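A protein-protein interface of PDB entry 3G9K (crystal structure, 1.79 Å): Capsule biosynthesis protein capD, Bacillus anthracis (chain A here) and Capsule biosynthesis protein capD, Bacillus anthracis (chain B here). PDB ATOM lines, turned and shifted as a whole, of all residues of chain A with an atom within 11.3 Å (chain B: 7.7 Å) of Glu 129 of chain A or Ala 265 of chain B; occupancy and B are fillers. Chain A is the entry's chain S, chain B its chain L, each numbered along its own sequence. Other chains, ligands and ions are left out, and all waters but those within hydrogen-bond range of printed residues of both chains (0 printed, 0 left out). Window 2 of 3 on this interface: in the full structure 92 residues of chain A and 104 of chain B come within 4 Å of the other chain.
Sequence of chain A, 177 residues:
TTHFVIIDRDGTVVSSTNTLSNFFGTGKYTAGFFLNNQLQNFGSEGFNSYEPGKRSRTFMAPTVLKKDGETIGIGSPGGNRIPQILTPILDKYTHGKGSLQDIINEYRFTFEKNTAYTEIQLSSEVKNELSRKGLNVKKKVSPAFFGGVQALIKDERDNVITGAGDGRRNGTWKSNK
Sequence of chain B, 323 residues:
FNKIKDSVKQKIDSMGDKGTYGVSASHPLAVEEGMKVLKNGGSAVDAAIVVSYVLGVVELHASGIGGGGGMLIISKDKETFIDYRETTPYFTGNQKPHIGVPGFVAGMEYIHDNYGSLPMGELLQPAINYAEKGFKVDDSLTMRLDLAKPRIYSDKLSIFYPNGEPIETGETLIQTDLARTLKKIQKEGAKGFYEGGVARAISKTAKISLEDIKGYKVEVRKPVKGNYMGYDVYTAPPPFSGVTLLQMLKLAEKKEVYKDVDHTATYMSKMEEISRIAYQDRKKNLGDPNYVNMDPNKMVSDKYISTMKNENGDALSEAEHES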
ATOM      1  N   GLU A 106       5.063   0.994 -39.515  1.00  0.00           N
ATOM      2  CA  GLU A 106       5.291   0.168 -38.331  1.00  0.00           C
ATOM      3  C   GLU A 106       3.923  -0.217 -37.784  1.00  0.00           C
ATOM      4  O   GLU A 106       3.008   0.596 -37.800  1.00  0.00           O
ATOM      5  CB  GLU A 106       6.044   0.958 -37.260  1.00  0.00           C
ATOM      6  CG  GLU A 106       6.670   0.110 -36.165  1.00  0.00           C
ATOM      7  CD  GLU A 106       7.699   0.837 -35.281  1.00  0.00           C
ATOM      8  OE1 GLU A 106       7.915   2.058 -35.383  1.00  0.00           O
ATOM      9  OE2 GLU A 106       8.320   0.135 -34.448  1.00  0.00           O
ATOM     10  N   PHE A 109      -0.339   0.226 -31.860  1.00  0.00           N
ATOM     11  CA  PHE A 109      -1.139  -0.165 -30.693  1.00  0.00           C
ATOM     12  C   PHE A 109      -1.888   1.031 -30.136  1.00  0.00           C
ATOM     13  O   PHE A 109      -1.398   2.166 -30.192  1.00  0.00           O
ATOM     14  CB  PHE A 109      -0.237  -0.733 -29.590  1.00  0.00           C
ATOM     15  CG  PHE A 109       0.807   0.233 -29.113  1.00  0.00           C
ATOM     16  CD1 PHE A 109       2.064   0.249 -29.698  1.00  0.00           C
ATOM     17  CD2 PHE A 109       0.537   1.125 -28.107  1.00  0.00           C
ATOM     18  CE1 PHE A 109       3.029   1.144 -29.276  1.00  0.00           C
ATOM     19  CE2 PHE A 109       1.485   2.031 -27.682  1.00  0.00           C
ATOM     20  CZ  PHE A 109       2.741   2.036 -28.263  1.00  0.00           C
ATOM     21  N   PHE A 111      -4.892   2.049 -26.681  1.00  0.00           N
ATOM     22  CA  PHE A 111      -5.444   1.621 -25.399  1.00  0.00           C
ATOM     23  C   PHE A 111      -6.874   2.094 -25.214  1.00  0.00           C
ATOM     24  O   PHE A 111      -7.225   3.206 -25.598  1.00  0.00           O
ATOM     25  CB  PHE A 111      -4.568   2.136 -24.280  1.00  0.00           C
ATOM     26  CG  PHE A 111      -3.204   1.539 -24.293  1.00  0.00           C
ATOM     27  CD1 PHE A 111      -2.162   2.169 -24.958  1.00  0.00           C
ATOM     28  CD2 PHE A 111      -2.969   0.317 -23.693  1.00  0.00           C
ATOM     29  CE1 PHE A 111      -0.903   1.608 -24.985  1.00  0.00           C
ATOM     30  CE2 PHE A 111      -1.714  -0.238 -23.718  1.00  0.00           C
ATOM     31  CZ  PHE A 111      -0.679   0.418 -24.370  1.00  0.00           C
ATOM     32  N   ASN A 114      -8.538  -0.597 -19.768  1.00  0.00           N
ATOM     33  CA  ASN A 114      -7.433  -1.476 -19.428  1.00  0.00           C
ATOM     34  C   ASN A 114      -6.920  -2.392 -20.544  1.00  0.00           C
ATOM     35  O   ASN A 114      -6.038  -3.141 -20.323  1.00  0.00           O
ATOM     36  CB  ASN A 114      -7.793  -2.290 -18.191  1.00  0.00           C
ATOM     37  CG  ASN A 114      -6.636  -2.523 -17.310  1.00  0.00           C
ATOM     38  OD1 ASN A 114      -5.875  -1.617 -17.008  1.00  0.00           O
ATOM     39  ND2 ASN A 114      -6.479  -3.766 -16.877  1.00  0.00           N
ATOM     40  N   ALA A 116      -5.075  -3.206 -24.292  1.00  0.00           N
ATOM     41  CA  ALA A 116      -4.157  -2.731 -25.313  1.00  0.00           C
ATOM     42  C   ALA A 116      -4.547  -3.423 -26.622  1.00  0.00           C
ATOM     43  O   ALA A 116      -4.510  -4.646 -26.733  1.00  0.00           O
ATOM     44  CB  ALA A 116      -2.727  -3.034 -24.930  1.00  0.00           C
ATOM     45  N   THR A 118      -3.760  -4.196 -30.428  1.00  0.00           N
ATOM     46  CA  THR A 118      -2.476  -4.396 -31.064  1.00  0.00           C
ATOM     47  C   THR A 118      -2.746  -4.821 -32.497  1.00  0.00           C
ATOM     48  O   THR A 118      -3.652  -5.595 -32.759  1.00  0.00           O
ATOM     49  CB  THR A 118      -1.650  -5.485 -30.309  1.00  0.00           C
ATOM     50  OG1 THR A 118      -1.100  -4.924 -29.091  1.00  0.00           O
ATOM     51  CG2 THR A 118      -0.564  -5.973 -31.161  1.00  0.00           C
ATOM     52  N   LEU A 122       1.352 -10.081 -30.507  1.00  0.00           N
ATOM     53  CA  LEU A 122       2.519  -9.912 -29.638  1.00  0.00           C
ATOM     54  C   LEU A 122       2.969 -11.230 -28.972  1.00  0.00           C
ATOM     55  O   LEU A 122       2.178 -12.161 -28.790  1.00  0.00           O
ATOM     56  CB  LEU A 122       2.235  -8.890 -28.541  1.00  0.00           C
ATOM     57  CG  LEU A 122       2.033  -7.418 -28.911  1.00  0.00           C
ATOM     58  CD1 LEU A 122       2.310  -6.565 -27.679  1.00  0.00           C
ATOM     59  CD2 LEU A 122       2.916  -6.965 -30.063  1.00  0.00           C
ATOM     60  N   SER A 123       4.239 -11.272 -28.592  1.00  0.00           N
ATOM     61  CA  SER A 123       4.826 -12.423 -27.911  1.00  0.00           C
ATOM     62  C   SER A 123       4.193 -12.649 -26.539  1.00  0.00           C
ATOM     63  O   SER A 123       3.647 -11.721 -25.931  1.00  0.00           O
ATOM     64  CB  SER A 123       6.325 -12.190 -27.707  1.00  0.00           C
ATOM     65  OG  SER A 123       6.535 -11.169 -26.738  1.00  0.00           O
ATOM     66  N   SER A 124       4.273 -13.886 -26.050  1.00  0.00           N
ATOM     67  CA  SER A 124       3.900 -14.195 -24.670  1.00  0.00           C
ATOM     68  C   SER A 124       4.813 -13.411 -23.724  1.00  0.00           C
ATOM     69  O   SER A 124       4.391 -12.963 -22.662  1.00  0.00           O
ATOM     70  CB  SER A 124       3.992 -15.710 -24.418  1.00  0.00           C
ATOM     71  OG  SER A 124       5.011 -16.307 -25.210  1.00  0.00           O
ATOM     72  N   GLU A 125       6.060 -13.232 -24.148  1.00  0.00           N
ATOM     73  CA  GLU A 125       7.060 -12.434 -23.430  1.00  0.00           C
ATOM     74  C   GLU A 125       6.568 -11.019 -23.066  1.00  0.00           C
ATOM     75  O   GLU A 125       6.567 -10.626 -21.893  1.00  0.00           O
ATOM     76  CB  GLU A 125       8.363 -12.405 -24.271  1.00  0.00           C
ATOM     77  CG  GLU A 125       9.255 -11.163 -24.155  1.00  0.00           C
ATOM     78  CD  GLU A 125       9.967 -11.056 -22.817  1.00  0.00           C
ATOM     79  OE1 GLU A 125      10.612 -12.049 -22.398  1.00  0.00           O
ATOM     80  OE2 GLU A 125       9.903  -9.971 -22.196  1.00  0.00           O
ATOM     81  N   VAL A 126       6.149 -10.253 -24.072  1.00  0.00           N
ATOM     82  CA  VAL A 126       5.697  -8.878 -23.840  1.00  0.00           C
ATOM     83  C   VAL A 126       4.284  -8.855 -23.268  1.00  0.00           C
ATOM     84  O   VAL A 126       3.969  -8.002 -22.448  1.00  0.00           O
ATOM     85  CB  VAL A 126       5.756  -8.022 -25.123  1.00  0.00           C
ATOM     86  CG1 VAL A 126       7.191  -7.959 -25.664  1.00  0.00           C
ATOM     87  CG2 VAL A 126       4.804  -8.568 -26.165  1.00  0.00           C
ATOM     88  N   LYS A 127       3.440  -9.791 -23.701  1.00  0.00           N
ATOM     89  CA  LYS A 127       2.083  -9.907 -23.170  1.00  0.00           C
ATOM     90  C   LYS A 127       2.089 -10.009 -21.648  1.00  0.00           C
ATOM     91  O   LYS A 127       1.332  -9.298 -20.976  1.00  0.00           O
ATOM     92  CB  LYS A 127       1.351 -11.123 -23.752  1.00  0.00           C
ATOM     93  CG  LYS A 127       0.610 -10.872 -25.049  1.00  0.00           C
ATOM     94  CD  LYS A 127      -0.361 -12.008 -25.342  1.00  0.00           C
ATOM     95  CE  LYS A 127      -1.051 -11.835 -26.691  1.00  0.00           C
ATOM     96  NZ  LYS A 127      -1.725 -13.090 -27.127  1.00  0.00           N
ATOM     97  N   ASN A 128       2.942 -10.884 -21.110  1.00  0.00           N
ATOM     98  CA  ASN A 128       3.018 -11.086 -19.655  1.00  0.00           C
ATOM     99  C   ASN A 128       3.552  -9.871 -18.888  1.00  0.00           C
ATOM    100  O   ASN A 128       3.097  -9.597 -17.776  1.00  0.00           O
ATOM    101  CB  ASN A 128       3.834 -12.339 -19.314  1.00  0.00           C
ATOM    102  CG  ASN A 128       3.239 -13.604 -19.920  1.00  0.00           C
ATOM    103  OD1 ASN A 128       2.017 -13.751 -20.025  1.00  0.00           O
ATOM    104  ND2 ASN A 128       4.108 -14.516 -20.345  1.00  0.00           N
ATOM    105  N   GLU A 129       4.499  -9.138 -19.473  1.00  0.00           N
ATOM    106  CA  GLU A 129       4.929  -7.858 -18.897  1.00  0.00           C
ATOM    107  C   GLU A 129       3.755  -6.897 -18.747  1.00  0.00           C
ATOM    108  O   GLU A 129       3.617  -6.212 -17.726  1.00  0.00           O
ATOM    109  CB  GLU A 129       5.995  -7.192 -19.753  1.00  0.00           C
ATOM    110  CG  GLU A 129       7.368  -7.780 -19.592  1.00  0.00           C
ATOM    111  CD  GLU A 129       8.444  -6.911 -20.215  1.00  0.00           C
ATOM    112  OE1 GLU A 129       8.669  -5.786 -19.705  1.00  0.00           O
ATOM    113  OE2 GLU A 129       9.068  -7.366 -21.207  1.00  0.00           O
ATOM    114  N   LEU A 130       2.920  -6.845 -19.782  1.00  0.00           N
ATOM    115  CA  LEU A 130       1.737  -5.995 -19.778  1.00  0.00           C
ATOM    116  C   LEU A 130       0.671  -6.563 -18.843  1.00  0.00           C
ATOM    117  O   LEU A 130      -0.044  -5.801 -18.199  1.00  0.00           O
ATOM    118  CB  LEU A 130       1.182  -5.827 -21.202  1.00  0.00           C
ATOM    119  CG  LEU A 130       2.121  -5.128 -22.200  1.00  0.00           C
ATOM    120  CD1 LEU A 130       1.675  -5.345 -23.639  1.00  0.00           C
ATOM    121  CD2 LEU A 130       2.232  -3.641 -21.889  1.00  0.00           C
ATOM    122  N   SER A 131       0.582  -7.893 -18.763  1.00  0.00           N
ATOM    123  CA  SER A 131      -0.422  -8.568 -17.914  1.00  0.00           C
ATOM    124  C   SER A 131      -0.309  -8.226 -16.431  1.00  0.00           C
ATOM    125  O   SER A 131      -1.328  -8.077 -15.755  1.00  0.00           O
ATOM    126  CB  SER A 131      -0.364 -10.090 -18.087  1.00  0.00           C
ATOM    127  OG  SER A 131      -0.929 -10.484 -19.328  1.00  0.00           O
ATOM    128  N   ARG A 132       0.918  -8.092 -15.933  1.00  0.00           N
ATOM    129  CA  ARG A 132       1.133  -7.713 -14.537  1.00  0.00           C
ATOM    130  C   ARG A 132       1.192  -6.198 -14.374  1.00  0.00           C
ATOM    131  O   ARG A 132       1.576  -5.712 -13.309  1.00  0.00           O
ATOM    132  CB  ARG A 132       2.447  -8.271 -13.975  1.00  0.00           C
ATOM    133  CG  ARG A 132       2.889  -9.673 -14.416  1.00  0.00           C
ATOM    134  CD  ARG A 132       4.425  -9.758 -14.497  1.00  0.00           C
ATOM    135  NE  ARG A 132       5.005  -8.650 -15.275  1.00  0.00           N
ATOM    136  CZ  ARG A 132       5.456  -7.493 -14.771  1.00  0.00           C
ATOM    137  NH1 ARG A 132       5.430  -7.250 -13.460  1.00  0.00           N
ATOM    138  NH2 ARG A 132       5.938  -6.556 -15.588  1.00  0.00           N
ATOM    139  N   LYS A 133       0.869  -5.451 -15.425  1.00  0.00           N
ATOM    140  CA  LYS A 133       0.928  -3.988 -15.366  1.00  0.00           C
ATOM    141  C   LYS A 133      -0.325  -3.213 -14.883  1.00  0.00           C
ATOM    142  O   LYS A 133      -0.155  -2.111 -14.355  1.00  0.00           O
ATOM    143  CB  LYS A 133       1.439  -3.416 -16.699  1.00  0.00           C
ATOM    144  CG  LYS A 133       2.933  -3.090 -16.682  1.00  0.00           C
ATOM    145  CD  LYS A 133       3.214  -1.912 -15.734  1.00  0.00           C
ATOM    146  CE  LYS A 133       4.468  -1.130 -16.113  1.00  0.00           C
ATOM    147  NZ  LYS A 133       4.411   0.270 -15.591  1.00  0.00           N
ATOM    148  N   GLY A 134      -1.558  -3.715 -15.029  1.00  0.00           N
ATOM    149  CA  GLY A 134      -1.913  -4.962 -15.688  1.00  0.00           C
ATOM    150  C   GLY A 134      -2.853  -4.700 -16.846  1.00  0.00           C
ATOM    151  O   GLY A 134      -4.070  -4.720 -16.683  1.00  0.00           O
ATOM    152  N   LEU A 135      -2.275  -4.442 -18.016  1.00  0.00           N
ATOM    153  CA  LEU A 135      -3.036  -4.265 -19.252  1.00  0.00           C
ATOM    154  C   LEU A 135      -3.238  -5.633 -19.879  1.00  0.00           C
ATOM    155  O   LEU A 135      -2.318  -6.451 -19.870  1.00  0.00           O
ATOM    156  CB  LEU A 135      -2.274  -3.377 -20.255  1.00  0.00           C
ATOM    157  CG  LEU A 135      -1.938  -1.907 -19.952  1.00  0.00           C
ATOM    158  CD1 LEU A 135      -3.177  -1.113 -19.557  1.00  0.00           C
ATOM    159  CD2 LEU A 135      -0.851  -1.793 -18.897  1.00  0.00           C
ATOM    160  N   ASN A 136      -4.421  -5.889 -20.424  1.00  0.00           N
ATOM    161  CA  ASN A 136      -4.603  -7.084 -21.250  1.00  0.00           C
ATOM    162  C   ASN A 136      -4.557  -6.700 -22.727  1.00  0.00           C
ATOM    163  O   ASN A 136      -4.738  -5.536 -23.069  1.00  0.00           O
ATOM    164  CB  ASN A 136      -5.860  -7.880 -20.872  1.00  0.00           C
ATOM    165  CG  ASN A 136      -7.140  -7.121 -21.104  1.00  0.00           C
ATOM    166  OD1 ASN A 136      -7.806  -7.317 -22.122  1.00  0.00           O
ATOM    167  ND2 ASN A 136      -7.514  -6.272 -20.151  1.00  0.00           N
ATOM    168  N   VAL A 137      -4.291  -7.677 -23.588  1.00  0.00           N
ATOM    169  CA  VAL A 137      -3.908  -7.410 -24.973  1.00  0.00           C
ATOM    170  C   VAL A 137      -4.805  -8.159 -25.944  1.00  0.00           C
ATOM    171  O   VAL A 137      -5.080  -9.336 -25.750  1.00  0.00           O
ATOM    172  CB  VAL A 137      -2.437  -7.799 -25.209  1.00  0.00           C
ATOM    173  CG1 VAL A 137      -2.064  -7.655 -26.664  1.00  0.00           C
ATOM    174  CG2 VAL A 137      -1.521  -6.942 -24.336  1.00  0.00           C
ATOM    175  N   ASP B 260      12.895   4.341 -24.344  1.00  0.00           N
ATOM    176  CA  ASP B 260      12.379   2.959 -24.249  1.00  0.00           C
ATOM    177  C   ASP B 260      11.817   2.375 -25.552  1.00  0.00           C
ATOM    178  O   ASP B 260      11.172   1.325 -25.519  1.00  0.00           O
ATOM    179  CB  ASP B 260      11.269   2.894 -23.197  1.00  0.00           C
ATOM    180  CG  ASP B 260      11.676   3.514 -21.877  1.00  0.00           C
ATOM    181  OD1 ASP B 260      12.632   3.012 -21.253  1.00  0.00           O
ATOM    182  OD2 ASP B 260      11.036   4.504 -21.463  1.00  0.00           O
ATOM    183  N   VAL B 261      12.056   3.021 -26.694  1.00  0.00           N
ATOM    184  CA  VAL B 261      11.372   2.624 -27.942  1.00  0.00           C
ATOM    185  C   VAL B 261      11.693   1.184 -28.396  1.00  0.00           C
ATOM    186  O   VAL B 261      10.866   0.519 -29.024  1.00  0.00           O
ATOM    187  CB  VAL B 261      11.636   3.632 -29.104  1.00  0.00           C
ATOM    188  CG1 VAL B 261      13.097   3.594 -29.553  1.00  0.00           C
ATOM    189  CG2 VAL B 261      10.708   3.347 -30.276  1.00  0.00           C
ATOM    190  N   ASP B 262      12.889   0.708 -28.072  1.00  0.00           N
ATOM    191  CA  ASP B 262      13.282  -0.672 -28.388  1.00  0.00           C
ATOM    192  C   ASP B 262      12.763  -1.700 -27.384  1.00  0.00           C
ATOM    193  O   ASP B 262      12.928  -2.899 -27.602  1.00  0.00           O
ATOM    194  CB  ASP B 262      14.811  -0.788 -28.468  1.00  0.00           C
ATOM    195  CG  ASP B 262      15.413   0.093 -29.547  1.00  0.00           C
ATOM    196  OD1 ASP B 262      14.717   0.412 -30.536  1.00  0.00           O
ATOM    197  OD2 ASP B 262      16.592   0.461 -29.396  1.00  0.00           O
ATOM    198  N   HIS B 263      12.149  -1.241 -26.300  1.00  0.00           N
ATOM    199  CA  HIS B 263      11.647  -2.121 -25.254  1.00  0.00           C
ATOM    200  C   HIS B 263      10.110  -2.043 -25.144  1.00  0.00           C
ATOM    201  O   HIS B 263       9.550  -1.269 -24.352  1.00  0.00           O
ATOM    202  CB  HIS B 263      12.347  -1.771 -23.944  1.00  0.00           C
ATOM    203  CG  HIS B 263      13.823  -2.015 -23.989  1.00  0.00           C
ATOM    204  ND1 HIS B 263      14.366  -3.284 -23.977  1.00  0.00           N
ATOM    205  CD2 HIS B 263      14.871  -1.159 -24.080  1.00  0.00           C
ATOM    206  CE1 HIS B 263      15.683  -3.200 -24.042  1.00  0.00           C
ATOM    207  NE2 HIS B 263      16.015  -1.921 -24.107  1.00  0.00           N
ATOM    208  N   THR B 264       9.451  -2.888 -25.936  1.00  0.00           N
ATOM    209  CA  THR B 264       8.038  -2.724 -26.292  1.00  0.00           C
ATOM    210  C   THR B 264       7.050  -2.593 -25.131  1.00  0.00           C
ATOM    211  O   THR B 264       6.223  -1.669 -25.116  1.00  0.00           O
ATOM    212  CB  THR B 264       7.603  -3.868 -27.213  1.00  0.00           C
ATOM    213  OG1 THR B 264       8.464  -3.872 -28.355  1.00  0.00           O
ATOM    214  CG2 THR B 264       6.160  -3.701 -27.664  1.00  0.00           C
ATOM    215  N   ALA B 265       7.133  -3.501 -24.157  1.00  0.00           N
ATOM    216  CA  ALA B 265       6.233  -3.439 -23.011  1.00  0.00           C
ATOM    217  C   ALA B 265       6.384  -2.111 -22.254  1.00  0.00           C
ATOM    218  O   ALA B 265       5.399  -1.563 -21.759  1.00  0.00           O
ATOM    219  CB  ALA B 265       6.469  -4.626 -22.074  1.00  0.00           C
ATOM    220  N   THR B 266       7.609  -1.588 -22.170  1.00  0.00           N
ATOM    221  CA  THR B 266       7.841  -0.320 -21.476  1.00  0.00           C
ATOM    222  C   THR B 266       7.283   0.851 -22.287  1.00  0.00           C
ATOM    223  O   THR B 266       6.644   1.757 -21.750  1.00  0.00           O
ATOM    224  CB  THR B 266       9.342  -0.059 -21.226  1.00  0.00           C
ATOM    225  OG1 THR B 266       9.937  -1.207 -20.619  1.00  0.00           O
ATOM    226  CG2 THR B 266       9.551   1.158 -20.323  1.00  0.00           C
ATOM    227  N   TYR B 267       7.560   0.827 -23.588  1.00  0.00           N
ATOM    228  CA  TYR B 267       7.097   1.873 -24.484  1.00  0.00           C
ATOM    229  C   TYR B 267       5.581   1.931 -24.438  1.00  0.00           C
ATOM    230  O   TYR B 267       5.015   3.006 -24.238  1.00  0.00           O
ATOM    231  CB  TYR B 267       7.589   1.641 -25.923  1.00  0.00           C
ATOM    232  CG  TYR B 267       7.440   2.868 -26.830  1.00  0.00           C
ATOM    233  CD1 TYR B 267       8.211   4.012 -26.615  1.00  0.00           C
ATOM    234  CD2 TYR B 267       6.543   2.876 -27.911  1.00  0.00           C
ATOM    235  CE1 TYR B 267       8.095   5.138 -27.435  1.00  0.00           C
ATOM    236  CE2 TYR B 267       6.418   4.011 -28.755  1.00  0.00           C
ATOM    237  CZ  TYR B 267       7.190   5.138 -28.500  1.00  0.00           C
ATOM    238  OH  TYR B 267       7.106   6.273 -29.305  1.00  0.00           O
ATOM    239  N   MET B 268       4.950   0.770 -24.581  1.00  0.00           N
ATOM    240  CA  MET B 268       3.488   0.694 -24.606  1.00  0.00           C
ATOM    241  C   MET B 268       2.874   1.149 -23.293  1.00  0.00           C
ATOM    242  O   MET B 268       1.934   1.948 -23.287  1.00  0.00           O
ATOM    243  CB  MET B 268       3.009  -0.720 -24.949  1.00  0.00           C
ATOM    244  CG  MET B 268       3.247  -1.117 -26.387  1.00  0.00           C
ATOM    245  SD  MET B 268       2.692  -2.930 -26.795  1.00  0.00           S
ATOM    246  CE  MET B 268       0.800  -2.779 -26.466  1.00  0.00           C
ATOM    247  N   SER B 269       3.440   0.662 -22.227  1.00  0.00           N
ATOM    248  CA  SER B 269       2.902   1.013 -20.929  1.00  0.00           C
ATOM    249  C   SER B 269       3.033   2.520 -20.657  1.00  0.00           C
ATOM    250  O   SER B 269       2.098   3.134 -20.162  1.00  0.00           O
ATOM    251  CB  SER B 269       3.561   0.178 -19.820  1.00  0.00           C
ATOM    252  OG  SER B 269       3.022   0.546 -18.565  1.00  0.00           O
ATOM    253  N   LYS B 270       4.157   3.098 -21.029  1.00  0.00           N
ATOM    254  CA  LYS B 270       4.400   4.510 -20.809  1.00  0.00           C
ATOM    255  C   LYS B 270       3.498   5.376 -21.694  1.00  0.00           C
ATOM    256  O   LYS B 270       3.208   6.482 -21.380  1.00  0.00           O
ATOM    257  CB  LYS B 270       5.871   4.837 -21.036  1.00  0.00           C
ATOM    258  CG  LYS B 270       6.791   4.536 -19.846  1.00  0.00           C
ATOM    259  CD  LYS B 270       8.218   4.919 -20.116  1.00  0.00           C
ATOM    260  CE  LYS B 270       9.072   5.016 -18.844  1.00  0.00           C
ATOM    261  NZ  LYS B 270      10.419   5.560 -19.064  1.00  0.00           N
ATOM    262  N   MET B 271       3.160   4.866 -22.911  1.00  0.00           N
ATOM    263  CA  MET B 271       2.243   5.550 -23.823  1.00  0.00           C
ATOM    264  C   MET B 271       0.813   5.472 -23.297  1.00  0.00           C
ATOM    265  O   MET B 271       0.046   6.437 -23.419  1.00  0.00           O
ATOM    266  CB  MET B 271       2.330   4.974 -25.245  1.00  0.00           C
ATOM    267  CG  MET B 271       3.465   5.545 -26.092  1.00  0.00           C
ATOM    268  SD  MET B 271       3.388   7.502 -26.257  1.00  0.00           S
ATOM    269  CE  MET B 271       4.997   7.750 -27.304  1.00  0.00           C
ATOM    270  N   GLU B 273       0.021   5.453 -20.268  1.00  0.00           N
ATOM    271  CA  GLU B 273      -0.059   6.378 -19.151  1.00  0.00           C
ATOM    272  C   GLU B 273      -0.284   7.799 -19.669  1.00  0.00           C
ATOM    273  O   GLU B 273      -1.194   8.482 -19.213  1.00  0.00           O
ATOM    274  CB  GLU B 273       1.208   6.280 -18.284  1.00  0.00           C
ATOM    275  CG  GLU B 273       1.394   4.907 -17.608  1.00  0.00           C
ATOM    276  CD  GLU B 273       2.832   4.661 -17.123  1.00  0.00           C
ATOM    277  OE1 GLU B 273       3.482   5.624 -16.662  1.00  0.00           O
ATOM    278  OE2 GLU B 273       3.309   3.503 -17.194  1.00  0.00           O
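CD2 of Tyr 267 of chain B touches CZ of Phe 109 of chain A, at 3.9 Å.
Phe 109 of chain A touches Met 268 of chain B (CE1 to CG, 3.7 Å).
Phe 109 of chain A touches Met 271 of chain B.
Phe 111 of chain A touches Met 268 of chain B (CZ to O, 3.2 Å).
Met 268 of chain B touches Ala 116 of chain A.
OG1 of Thr 118 of chain A touches CE of Met 268 of chain B, at 3.9 Å.
CD1 of Leu 122 of chain A touches SD of Met 268 of chain B, at 3.8 Å.
OE1 of Glu 129 of chain A touches CB of Ala 265 of chain B, at 3.4 Å.
Ala 265 of chain B touches Leu 130 of chain A (O to CD2, 3.8 Å).
CD1 of Leu 130 of chain A touches CE of Met 268 of chain B, 3.9 Å away.
The backbone carbonyl oxygen of Leu 130 of chain A sits at hydrogen-bond distance from the backbone NH of Leu 135 of chain A.
O of Asn 136 of chain A sits at hydrogen-bond distance from N of Ala 116 of chain A (2.7 Å).
The backbone carbonyl oxygen (O) of Glu 129 of chain A is in hydrogen-bond range of the guanidinium group (NH2) of Arg 132 of chain A.
The side-chain hydroxyl (OG) of Ser 269 of chain B is in hydrogen-bond range of the side-chain carboxylate (OE2) of Glu 273 of chain B (3.3 Å).
Printed residues of chain A that touch a printed residue of chain B: Phe 109, Phe 111, Ala 116, Thr 118, Leu 122, Glu 129, Leu 130 and Lys 133.
Hydrophobic or aromatic side chains of chain A within 4 Å of the printed part of chain B: Phe 109, Phe 111, Ala 116, Leu 122 and Leu 130.
Among the printed residues, Asp or Glu carboxylates within 4 Å of a Lys or Arg side-chain nitrogen of the other chain: Lys 133 of chain A with Glu 273 of chain B.
The side-chain carboxylate (OE2) of Glu 273 of chain B is in salt-bridge range of the side-chain amino group (NZ) of Lys 133 of chain A (3.8 Å).
NZ of Lys 133 of chain A sits at hydrogen-bond distance from OG of Ser 269 of chain B, at 3.3 Å.
Of the printed residues of chain B, Phe 111 of chain A touches Met 268 (3.2 Å).
Printed residues of chain B within 4 Å of Leu 122 of chain A: Met 268 (3.8 Å).
Glu 129 of chain A touches one residue of chain B.
No residue of chain A comes within 4 Å of Thr 264 of chain B.
Ala 265 of chain B touches two residues of chain A.
Printed residues of chain A within 4 Å of Tyr 267 of chain B: Phe 109 (3.9 Å).
Of chain A, only Phe 109 (3.7 Å), Phe 111 (3.2 Å), Ala 116 (3.9 Å), Thr 118 (3.9 Å), Leu 122 (3.8 Å) and Leu 130 (3.9 Å) come within 4 Å of Met 268 of chain B.
Of the printed residues of chain A, Met 271 of chain B touches Phe 109 (3.9 Å).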
